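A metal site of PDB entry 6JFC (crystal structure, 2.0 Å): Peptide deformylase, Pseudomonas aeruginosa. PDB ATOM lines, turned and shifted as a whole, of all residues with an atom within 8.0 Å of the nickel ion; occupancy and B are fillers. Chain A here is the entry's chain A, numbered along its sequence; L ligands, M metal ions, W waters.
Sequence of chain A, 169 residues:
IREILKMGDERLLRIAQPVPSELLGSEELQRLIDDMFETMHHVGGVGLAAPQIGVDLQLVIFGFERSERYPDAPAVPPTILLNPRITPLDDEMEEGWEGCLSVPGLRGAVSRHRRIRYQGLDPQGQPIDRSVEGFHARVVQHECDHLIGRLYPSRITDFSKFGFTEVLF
SG of Cys 100 lies close to NE2 of Gln 52 (3.7 Å).
SG of Cys 100 sits close to N of Ser 102 (3.5 Å).
A ring nitrogen (ND1) of His 142 is in hydrogen-bond range of the side-chain carboxylate of Glu 98, 2.8 Å away.
The side-chain amide nitrogen (NE2) of Gln 52 is in hydrogen-bond range of the side-chain hydroxyl (OG) of Ser 102 (2.7 Å).
The side-chain amide oxygen (OE1) of Gln 52 sits at hydrogen-bond distance from the backbone NH (N) of Ala 49 (3.0 Å).
Merely in contact with the nickel ion: Gln 52 (3.7 Å).
Four residues have an atom within 4 Å of the nickel ion: Gln 52, Cys 100, His 142 and His 146.
The nearest printed residue that does not touch the nickel ion is Leu 101 (4.5 Å).
The side-chain sulfur of Cys 100 lies close to an oxygen (O1) of the ligand, at 3.8 Å.
A ring nitrogen (NE2) of His 146 sits close to an oxygen (O2) of the ligand, at 3.1 Å.
The side-chain amide oxygen (OE1) of Gln 52 lies within hydrogen-bond range of an oxygen (O2) of the ligand, at 2.5 Å.
O1 of the ligand lies within hydrogen-bond range of N of Leu 101 (3.1 Å).
An oxygen (O4) of the ligand lies within hydrogen-bond range of the backbone NH of Gly 99 (3.0 Å).
The backbone carbonyl oxygen (O) of Gly 99 is in hydrogen-bond range of a nitrogen (N2) of the ligand, at 3.2 Å.
The side-chain carboxylate of Glu 143 is in hydrogen-bond range of a nitrogen (N1) of the ligand, at 2.6 Å.
The backbone carbonyl oxygen (O) of Gly 47 lies close to a nitrogen (N1) of the ligand, at 3.2 Å.
The nickel ion is bound by SG of Cys 100 (2.1 Å), NE2 of His 142 (2.2 Å) and NE2 of His 146 (2.3 Å).
Slightly farther from the nickel ion lies O2 of the ligand (2.8 Å).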
ATOM      1  N   ILE A   4     -31.653 -15.810   2.642  1.00  0.00           N
ATOM      2  CA  ILE A   4     -30.745 -16.090   3.780  1.00  0.00           C
ATOM      3  C   ILE A   4     -29.895 -17.377   3.578  1.00  0.00           C
ATOM      4  O   ILE A   4     -30.423 -18.472   3.513  1.00  0.00           O
ATOM      5  CB  ILE A   4     -31.549 -16.101   5.091  1.00  0.00           C
ATOM      6  CG1 ILE A   4     -32.186 -14.721   5.298  1.00  0.00           C
ATOM      7  CG2 ILE A   4     -30.649 -16.341   6.314  1.00  0.00           C
ATOM      8  CD1 ILE A   4     -33.061 -14.631   6.540  1.00  0.00           C
ATOM      9  N   LEU A  12     -20.609 -17.835   4.636  1.00  0.00           N
ATOM     10  CA  LEU A  12     -20.829 -17.466   6.041  1.00  0.00           C
ATOM     11  C   LEU A  12     -19.549 -17.633   6.830  1.00  0.00           C
ATOM     12  O   LEU A  12     -19.552 -17.399   8.055  1.00  0.00           O
ATOM     13  CB  LEU A  12     -21.864 -18.407   6.682  1.00  0.00           C
ATOM     14  CG  LEU A  12     -23.259 -18.267   6.082  1.00  0.00           C
ATOM     15  CD1 LEU A  12     -24.275 -19.341   6.558  1.00  0.00           C
ATOM     16  CD2 LEU A  12     -23.786 -16.882   6.395  1.00  0.00           C
ATOM     17  N   GLY A  47     -31.946  -9.377  14.105  1.00  0.00           N
ATOM     18  CA  GLY A  47     -30.678  -8.886  13.537  1.00  0.00           C
ATOM     19  C   GLY A  47     -30.322  -9.563  12.243  1.00  0.00           C
ATOM     20  O   GLY A  47     -30.873 -10.614  11.913  1.00  0.00           O
ATOM     21  N   LEU A  48     -29.434  -8.961  11.478  1.00  0.00           N
ATOM     22  CA  LEU A  48     -29.039  -9.547  10.245  1.00  0.00           C
ATOM     23  C   LEU A  48     -27.753  -8.931   9.858  1.00  0.00           C
ATOM     24  O   LEU A  48     -27.536  -7.749  10.062  1.00  0.00           O
ATOM     25  CB  LEU A  48     -30.104  -9.336   9.137  1.00  0.00           C
ATOM     26  CG  LEU A  48     -29.931 -10.015   7.740  1.00  0.00           C
ATOM     27  CD1 LEU A  48     -29.996 -11.536   7.888  1.00  0.00           C
ATOM     28  CD2 LEU A  48     -30.957  -9.574   6.692  1.00  0.00           C
ATOM     29  N   ALA A  49     -26.882  -9.757   9.343  1.00  0.00           N
ATOM     30  CA  ALA A  49     -25.580  -9.306   8.919  1.00  0.00           C
ATOM     31  C   ALA A  49     -25.455  -9.475   7.396  1.00  0.00           C
ATOM     32  O   ALA A  49     -25.962 -10.464   6.837  1.00  0.00           O
ATOM     33  CB  ALA A  49     -24.505 -10.074   9.632  1.00  0.00           C
ATOM     34  N   GLN A  52     -24.895 -12.853   5.509  1.00  0.00           N
ATOM     35  CA  GLN A  52     -26.006 -13.806   5.509  1.00  0.00           C
ATOM     36  C   GLN A  52     -26.919 -13.754   4.240  1.00  0.00           C
ATOM     37  O   GLN A  52     -27.722 -14.688   3.975  1.00  0.00           O
ATOM     38  CB  GLN A  52     -26.897 -13.634   6.717  1.00  0.00           C
ATOM     39  CG  GLN A  52     -26.260 -13.995   8.047  1.00  0.00           C
ATOM     40  CD  GLN A  52     -27.219 -13.812   9.201  1.00  0.00           C
ATOM     41  OE1 GLN A  52     -27.383 -12.715   9.746  1.00  0.00           O
ATOM     42  NE2 GLN A  52     -27.826 -14.904   9.616  1.00  0.00           N
ATOM     43  N   GLU A  98     -29.681 -18.513  22.083  1.00  0.00           N
ATOM     44  CA  GLU A  98     -29.625 -17.907  20.783  1.00  0.00           C
ATOM     45  C   GLU A  98     -30.166 -18.855  19.750  1.00  0.00           C
ATOM     46  O   GLU A  98     -30.091 -20.047  19.899  1.00  0.00           O
ATOM     47  CB  GLU A  98     -28.199 -17.566  20.422  1.00  0.00           C
ATOM     48  CG  GLU A  98     -27.552 -16.716  21.496  1.00  0.00           C
ATOM     49  CD  GLU A  98     -26.227 -16.049  21.098  1.00  0.00           C
ATOM     50  OE1 GLU A  98     -25.736 -16.187  19.922  1.00  0.00           O
ATOM     51  OE2 GLU A  98     -25.645 -15.403  21.992  1.00  0.00           O
ATOM     52  N   GLY A  99     -30.719 -18.287  18.681  1.00  0.00           N
ATOM     53  CA  GLY A  99     -30.911 -18.998  17.437  1.00  0.00           C
ATOM     54  C   GLY A  99     -30.496 -18.043  16.356  1.00  0.00           C
ATOM     55  O   GLY A  99     -30.211 -16.899  16.632  1.00  0.00           O
ATOM     56  N   CYS A 100     -30.489 -18.505  15.115  1.00  0.00           N
ATOM     57  CA  CYS A 100     -29.965 -17.765  13.993  1.00  0.00           C
ATOM     58  C   CYS A 100     -30.781 -18.155  12.767  1.00  0.00           C
ATOM     59  O   CYS A 100     -31.133 -19.341  12.527  1.00  0.00           O
ATOM     60  CB  CYS A 100     -28.476 -18.074  13.820  1.00  0.00           C
ATOM     61  SG  CYS A 100     -27.551 -17.245  12.522  1.00  0.00           S
ATOM     62  N   LEU A 101     -31.051 -17.133  11.953  1.00  0.00           N
ATOM     63  CA  LEU A 101     -31.719 -17.289  10.681  1.00  0.00           C
ATOM     64  C   LEU A 101     -30.995 -18.263   9.792  1.00  0.00           C
ATOM     65  O   LEU A 101     -31.655 -19.040   9.101  1.00  0.00           O
ATOM     66  CB  LEU A 101     -31.833 -15.913   9.995  1.00  0.00           C
ATOM     67  CG  LEU A 101     -32.654 -14.936  10.880  1.00  0.00           C
ATOM     68  CD1 LEU A 101     -32.512 -13.506  10.416  1.00  0.00           C
ATOM     69  CD2 LEU A 101     -34.112 -15.357  10.921  1.00  0.00           C
ATOM     70  N   SER A 102     -29.666 -18.304   9.885  1.00  0.00           N
ATOM     71  CA  SER A 102     -28.846 -19.226   9.089  1.00  0.00           C
ATOM     72  C   SER A 102     -28.777 -20.677   9.615  1.00  0.00           C
ATOM     73  O   SER A 102     -28.161 -21.502   9.009  1.00  0.00           O
ATOM     74  CB  SER A 102     -27.427 -18.653   8.977  1.00  0.00           C
ATOM     75  OG  SER A 102     -27.518 -17.348   8.489  1.00  0.00           O
ATOM     76  N   VAL A 103     -29.380 -20.931  10.762  1.00  0.00           N
ATOM     77  CA  VAL A 103     -29.279 -22.206  11.441  1.00  0.00           C
ATOM     78  C   VAL A 103     -30.716 -22.580  11.814  1.00  0.00           C
ATOM     79  O   VAL A 103     -31.018 -22.785  12.985  1.00  0.00           O
ATOM     80  CB  VAL A 103     -28.435 -22.113  12.731  1.00  0.00           C
ATOM     81  CG1 VAL A 103     -28.266 -23.467  13.400  1.00  0.00           C
ATOM     82  CG2 VAL A 103     -27.049 -21.536  12.412  1.00  0.00           C
ATOM     83  N   ARG A 112     -21.723 -15.095  26.581  1.00  0.00           N
ATOM     84  CA  ARG A 112     -21.142 -13.880  25.963  1.00  0.00           C
ATOM     85  C   ARG A 112     -20.829 -12.845  27.043  1.00  0.00           C
ATOM     86  O   ARG A 112     -21.339 -12.929  28.163  1.00  0.00           O
ATOM     87  CB  ARG A 112     -22.106 -13.172  25.056  1.00  0.00           C
ATOM     88  CG  ARG A 112     -22.865 -14.004  24.050  1.00  0.00           C
ATOM     89  CD  ARG A 112     -22.206 -13.890  22.713  1.00  0.00           C
ATOM     90  NE  ARG A 112     -22.973 -14.527  21.638  1.00  0.00           N
ATOM     91  CZ  ARG A 112     -22.420 -14.808  20.462  1.00  0.00           C
ATOM     92  NH1 ARG A 112     -21.121 -14.501  20.232  1.00  0.00           N
ATOM     93  NH2 ARG A 112     -23.124 -15.412  19.536  1.00  0.00           N
ATOM     94  N   VAL A 139     -26.930  -9.294  21.236  1.00  0.00           N
ATOM     95  CA  VAL A 139     -27.305  -9.115  19.827  1.00  0.00           C
ATOM     96  C   VAL A 139     -26.098  -8.585  19.014  1.00  0.00           C
ATOM     97  O   VAL A 139     -25.753  -9.117  17.965  1.00  0.00           O
ATOM     98  CB  VAL A 139     -28.496  -8.157  19.694  1.00  0.00           C
ATOM     99  CG1 VAL A 139     -28.733  -7.804  18.270  1.00  0.00           C
ATOM    100  CG2 VAL A 139     -29.815  -8.816  20.248  1.00  0.00           C
ATOM    101  N   HIS A 142     -23.434 -11.370  18.656  1.00  0.00           N
ATOM    102  CA  HIS A 142     -23.882 -12.342  17.677  1.00  0.00           C
ATOM    103  C   HIS A 142     -23.688 -11.848  16.247  1.00  0.00           C
ATOM    104  O   HIS A 142     -23.134 -12.583  15.390  1.00  0.00           O
ATOM    105  CB  HIS A 142     -25.375 -12.671  17.951  1.00  0.00           C
ATOM    106  CG  HIS A 142     -25.947 -13.698  17.022  1.00  0.00           C
ATOM    107  ND1 HIS A 142     -26.184 -15.012  17.416  1.00  0.00           N
ATOM    108  CD2 HIS A 142     -26.430 -13.577  15.759  1.00  0.00           C
ATOM    109  CE1 HIS A 142     -26.763 -15.653  16.413  1.00  0.00           C
ATOM    110  NE2 HIS A 142     -26.928 -14.812  15.401  1.00  0.00           N
ATOM    111  N   GLU A 143     -24.165 -10.624  15.951  1.00  0.00           N
ATOM    112  CA  GLU A 143     -24.078 -10.061  14.615  1.00  0.00           C
ATOM    113  C   GLU A 143     -22.684  -9.813  14.172  1.00  0.00           C
ATOM    114  O   GLU A 143     -22.347 -10.127  13.026  1.00  0.00           O
ATOM    115  CB  GLU A 143     -24.859  -8.767  14.472  1.00  0.00           C
ATOM    116  CG  GLU A 143     -26.367  -8.874  14.585  1.00  0.00           C
ATOM    117  CD  GLU A 143     -26.968  -9.948  13.709  1.00  0.00           C
ATOM    118  OE1 GLU A 143     -26.468 -10.209  12.548  1.00  0.00           O
ATOM    119  OE2 GLU A 143     -27.926 -10.555  14.233  1.00  0.00           O
ATOM    120  N   ASP A 145     -20.067 -11.380  15.128  1.00  0.00           N
ATOM    121  CA  ASP A 145     -19.480 -12.708  14.851  1.00  0.00           C
ATOM    122  C   ASP A 145     -19.636 -13.151  13.401  1.00  0.00           C
ATOM    123  O   ASP A 145     -18.683 -13.704  12.818  1.00  0.00           O
ATOM    124  CB  ASP A 145     -20.042 -13.796  15.778  1.00  0.00           C
ATOM    125  CG  ASP A 145     -19.172 -14.085  16.967  1.00  0.00           C
ATOM    126  OD1 ASP A 145     -18.118 -13.419  17.119  1.00  0.00           O
ATOM    127  OD2 ASP A 145     -19.573 -14.975  17.782  1.00  0.00           O
ATOM    128  N   HIS A 146     -20.799 -12.873  12.790  1.00  0.00           N
ATOM    129  CA  HIS A 146     -20.981 -13.098  11.342  1.00  0.00           C
ATOM    130  C   HIS A 146     -19.910 -12.440  10.430  1.00  0.00           C
ATOM    131  O   HIS A 146     -19.538 -12.981   9.400  1.00  0.00           O
ATOM    132  CB  HIS A 146     -22.355 -12.678  10.854  1.00  0.00           C
ATOM    133  CG  HIS A 146     -23.456 -13.577  11.314  1.00  0.00           C
ATOM    134  ND1 HIS A 146     -23.646 -14.835  10.778  1.00  0.00           N
ATOM    135  CD2 HIS A 146     -24.484 -13.370  12.176  1.00  0.00           C
ATOM    136  CE1 HIS A 146     -24.712 -15.388  11.338  1.00  0.00           C
ATOM    137  NE2 HIS A 146     -25.228 -14.536  12.194  1.00  0.00           N
ATOM    138  N   ARG A 150     -18.026 -16.476  12.161  1.00  0.00           N
ATOM    139  CA  ARG A 150     -18.358 -17.321  13.332  1.00  0.00           C
ATOM    140  C   ARG A 150     -19.854 -17.407  13.468  1.00  0.00           C
ATOM    141  O   ARG A 150     -20.562 -16.390  13.502  1.00  0.00           O
ATOM    142  CB  ARG A 150     -17.705 -16.735  14.581  1.00  0.00           C
ATOM    143  CG  ARG A 150     -16.157 -16.714  14.551  1.00  0.00           C
ATOM    144  CD  ARG A 150     -15.524 -18.103  14.485  1.00  0.00           C
ATOM    145  NE  ARG A 150     -15.789 -18.836  15.726  1.00  0.00           N
ATOM    146  CZ  ARG A 150     -15.068 -18.755  16.851  1.00  0.00           C
ATOM    147  NH1 ARG A 150     -13.957 -17.980  16.948  1.00  0.00           N
ATOM    148  NH2 ARG A 150     -15.451 -19.452  17.901  1.00  0.00           N
ATOM    149  N   LEU A 151     -20.353 -18.605  13.471  1.00  0.00           N
ATOM    150  CA  LEU A 151     -21.724 -18.856  13.879  1.00  0.00           C
ATOM    151  C   LEU A 151     -21.822 -19.342  15.320  1.00  0.00           C
ATOM    152  O   LEU A 151     -20.891 -19.923  15.834  1.00  0.00           O
ATOM    153  CB  LEU A 151     -22.337 -19.869  12.922  1.00  0.00           C
ATOM    154  CG  LEU A 151     -22.467 -19.529  11.451  1.00  0.00           C
ATOM    155  CD1 LEU A 151     -23.313 -20.615  10.805  1.00  0.00           C
ATOM    156  CD2 LEU A 151     -23.181 -18.233  11.241  1.00  0.00           C
ATOM    157  N   TYR A 152     -22.981 -19.185  15.957  1.00  0.00           N
ATOM    158  CA  TYR A 152     -23.113 -19.522  17.391  1.00  0.00           C
ATOM    159  C   TYR A 152     -22.740 -20.975  17.787  1.00  0.00           C
ATOM    160  O   TYR A 152     -22.162 -21.185  18.848  1.00  0.00           O
ATOM    161  CB  TYR A 152     -24.455 -19.054  17.988  1.00  0.00           C
ATOM    162  CG  TYR A 152     -25.623 -20.005  17.764  1.00  0.00           C
ATOM    163  CD1 TYR A 152     -25.818 -21.059  18.548  1.00  0.00           C
ATOM    164  CD2 TYR A 152     -26.501 -19.813  16.712  1.00  0.00           C
ATOM    165  CE1 TYR A 152     -26.901 -21.938  18.350  1.00  0.00           C
ATOM    166  CE2 TYR A 152     -27.566 -20.675  16.516  1.00  0.00           C
ATOM    167  CZ  TYR A 152     -27.718 -21.782  17.297  1.00  0.00           C
ATOM    168  OH  TYR A 152     -28.792 -22.618  17.127  1.00  0.00           O
HETATM  169  C1  LIG L   1     -31.016 -13.176  13.690  1.00  0.00           C
HETATM  170  C2  LIG L   1     -29.808 -13.511  12.844  1.00  0.00           C
HETATM  171  O1  LIG L   1     -29.841 -14.328  11.931  1.00  0.00           O
HETATM  172  N1  LIG L   1     -28.746 -12.748  13.113  1.00  0.00           N
HETATM  173  O2  LIG L   1     -27.696 -12.700  12.264  1.00  0.00           O
HETATM  174  C3  LIG L   1     -30.929 -13.739  15.089  1.00  0.00           C
HETATM  175  C4  LIG L   1     -32.349 -13.850  15.548  1.00  0.00           C
HETATM  176  O3  LIG L   1     -33.131 -12.941  15.363  1.00  0.00           O
HETATM  177  C5  LIG L   1     -30.130 -12.841  16.056  1.00  0.00           C
HETATM  178  C6  LIG L   1     -30.362 -13.329  17.470  1.00  0.00           C
HETATM  179  C7  LIG L   1     -29.240 -13.019  18.419  1.00  0.00           C
HETATM  180  C8  LIG L   1     -29.393 -13.925  19.617  1.00  0.00           C
HETATM  181  C9  LIG L   1     -30.165 -13.170  20.668  1.00  0.00           C
HETATM  182  N2  LIG L   1     -32.660 -14.959  16.200  1.00  0.00           N
HETATM  183  C10 LIG L   1     -33.927 -15.135  16.873  1.00  0.00           C
HETATM  184  C11 LIG L   1     -34.792 -16.170  16.109  1.00  0.00           C
HETATM  185  C12 LIG L   1     -34.276 -16.539  14.712  1.00  0.00           C
HETATM  186  C13 LIG L   1     -35.000 -17.465  16.884  1.00  0.00           C
HETATM  187  C14 LIG L   1     -33.598 -15.364  18.348  1.00  0.00           C
HETATM  188  O4  LIG L   1     -32.538 -15.935  18.632  1.00  0.00           O
HETATM  189  N3  LIG L   1     -34.436 -14.909  19.300  1.00  0.00           N
HETATM  190  C15 LIG L   1     -33.983 -14.727  20.700  1.00  0.00           C
HETATM  191  C16 LIG L   1     -35.850 -14.502  19.186  1.00  0.00           C
HETATM  192  C17 LIG L   1     -35.953 -13.334  20.154  1.00  0.00           C
HETATM  193  C18 LIG L   1     -34.779 -13.487  21.118  1.00  0.00           C
HETATM  194  C19 LIG L   1     -34.354 -15.936  21.575  1.00  0.00           C
HETATM  195  O5  LIG L   1     -33.640 -17.134  21.202  1.00  0.00           O
HETATM  196 NI    NI M   1     -27.197 -15.248  13.216  1.00  0.00          NI
HETATM  197  O   HOH W   1     -24.789 -17.423  14.492  1.00  0.00           O
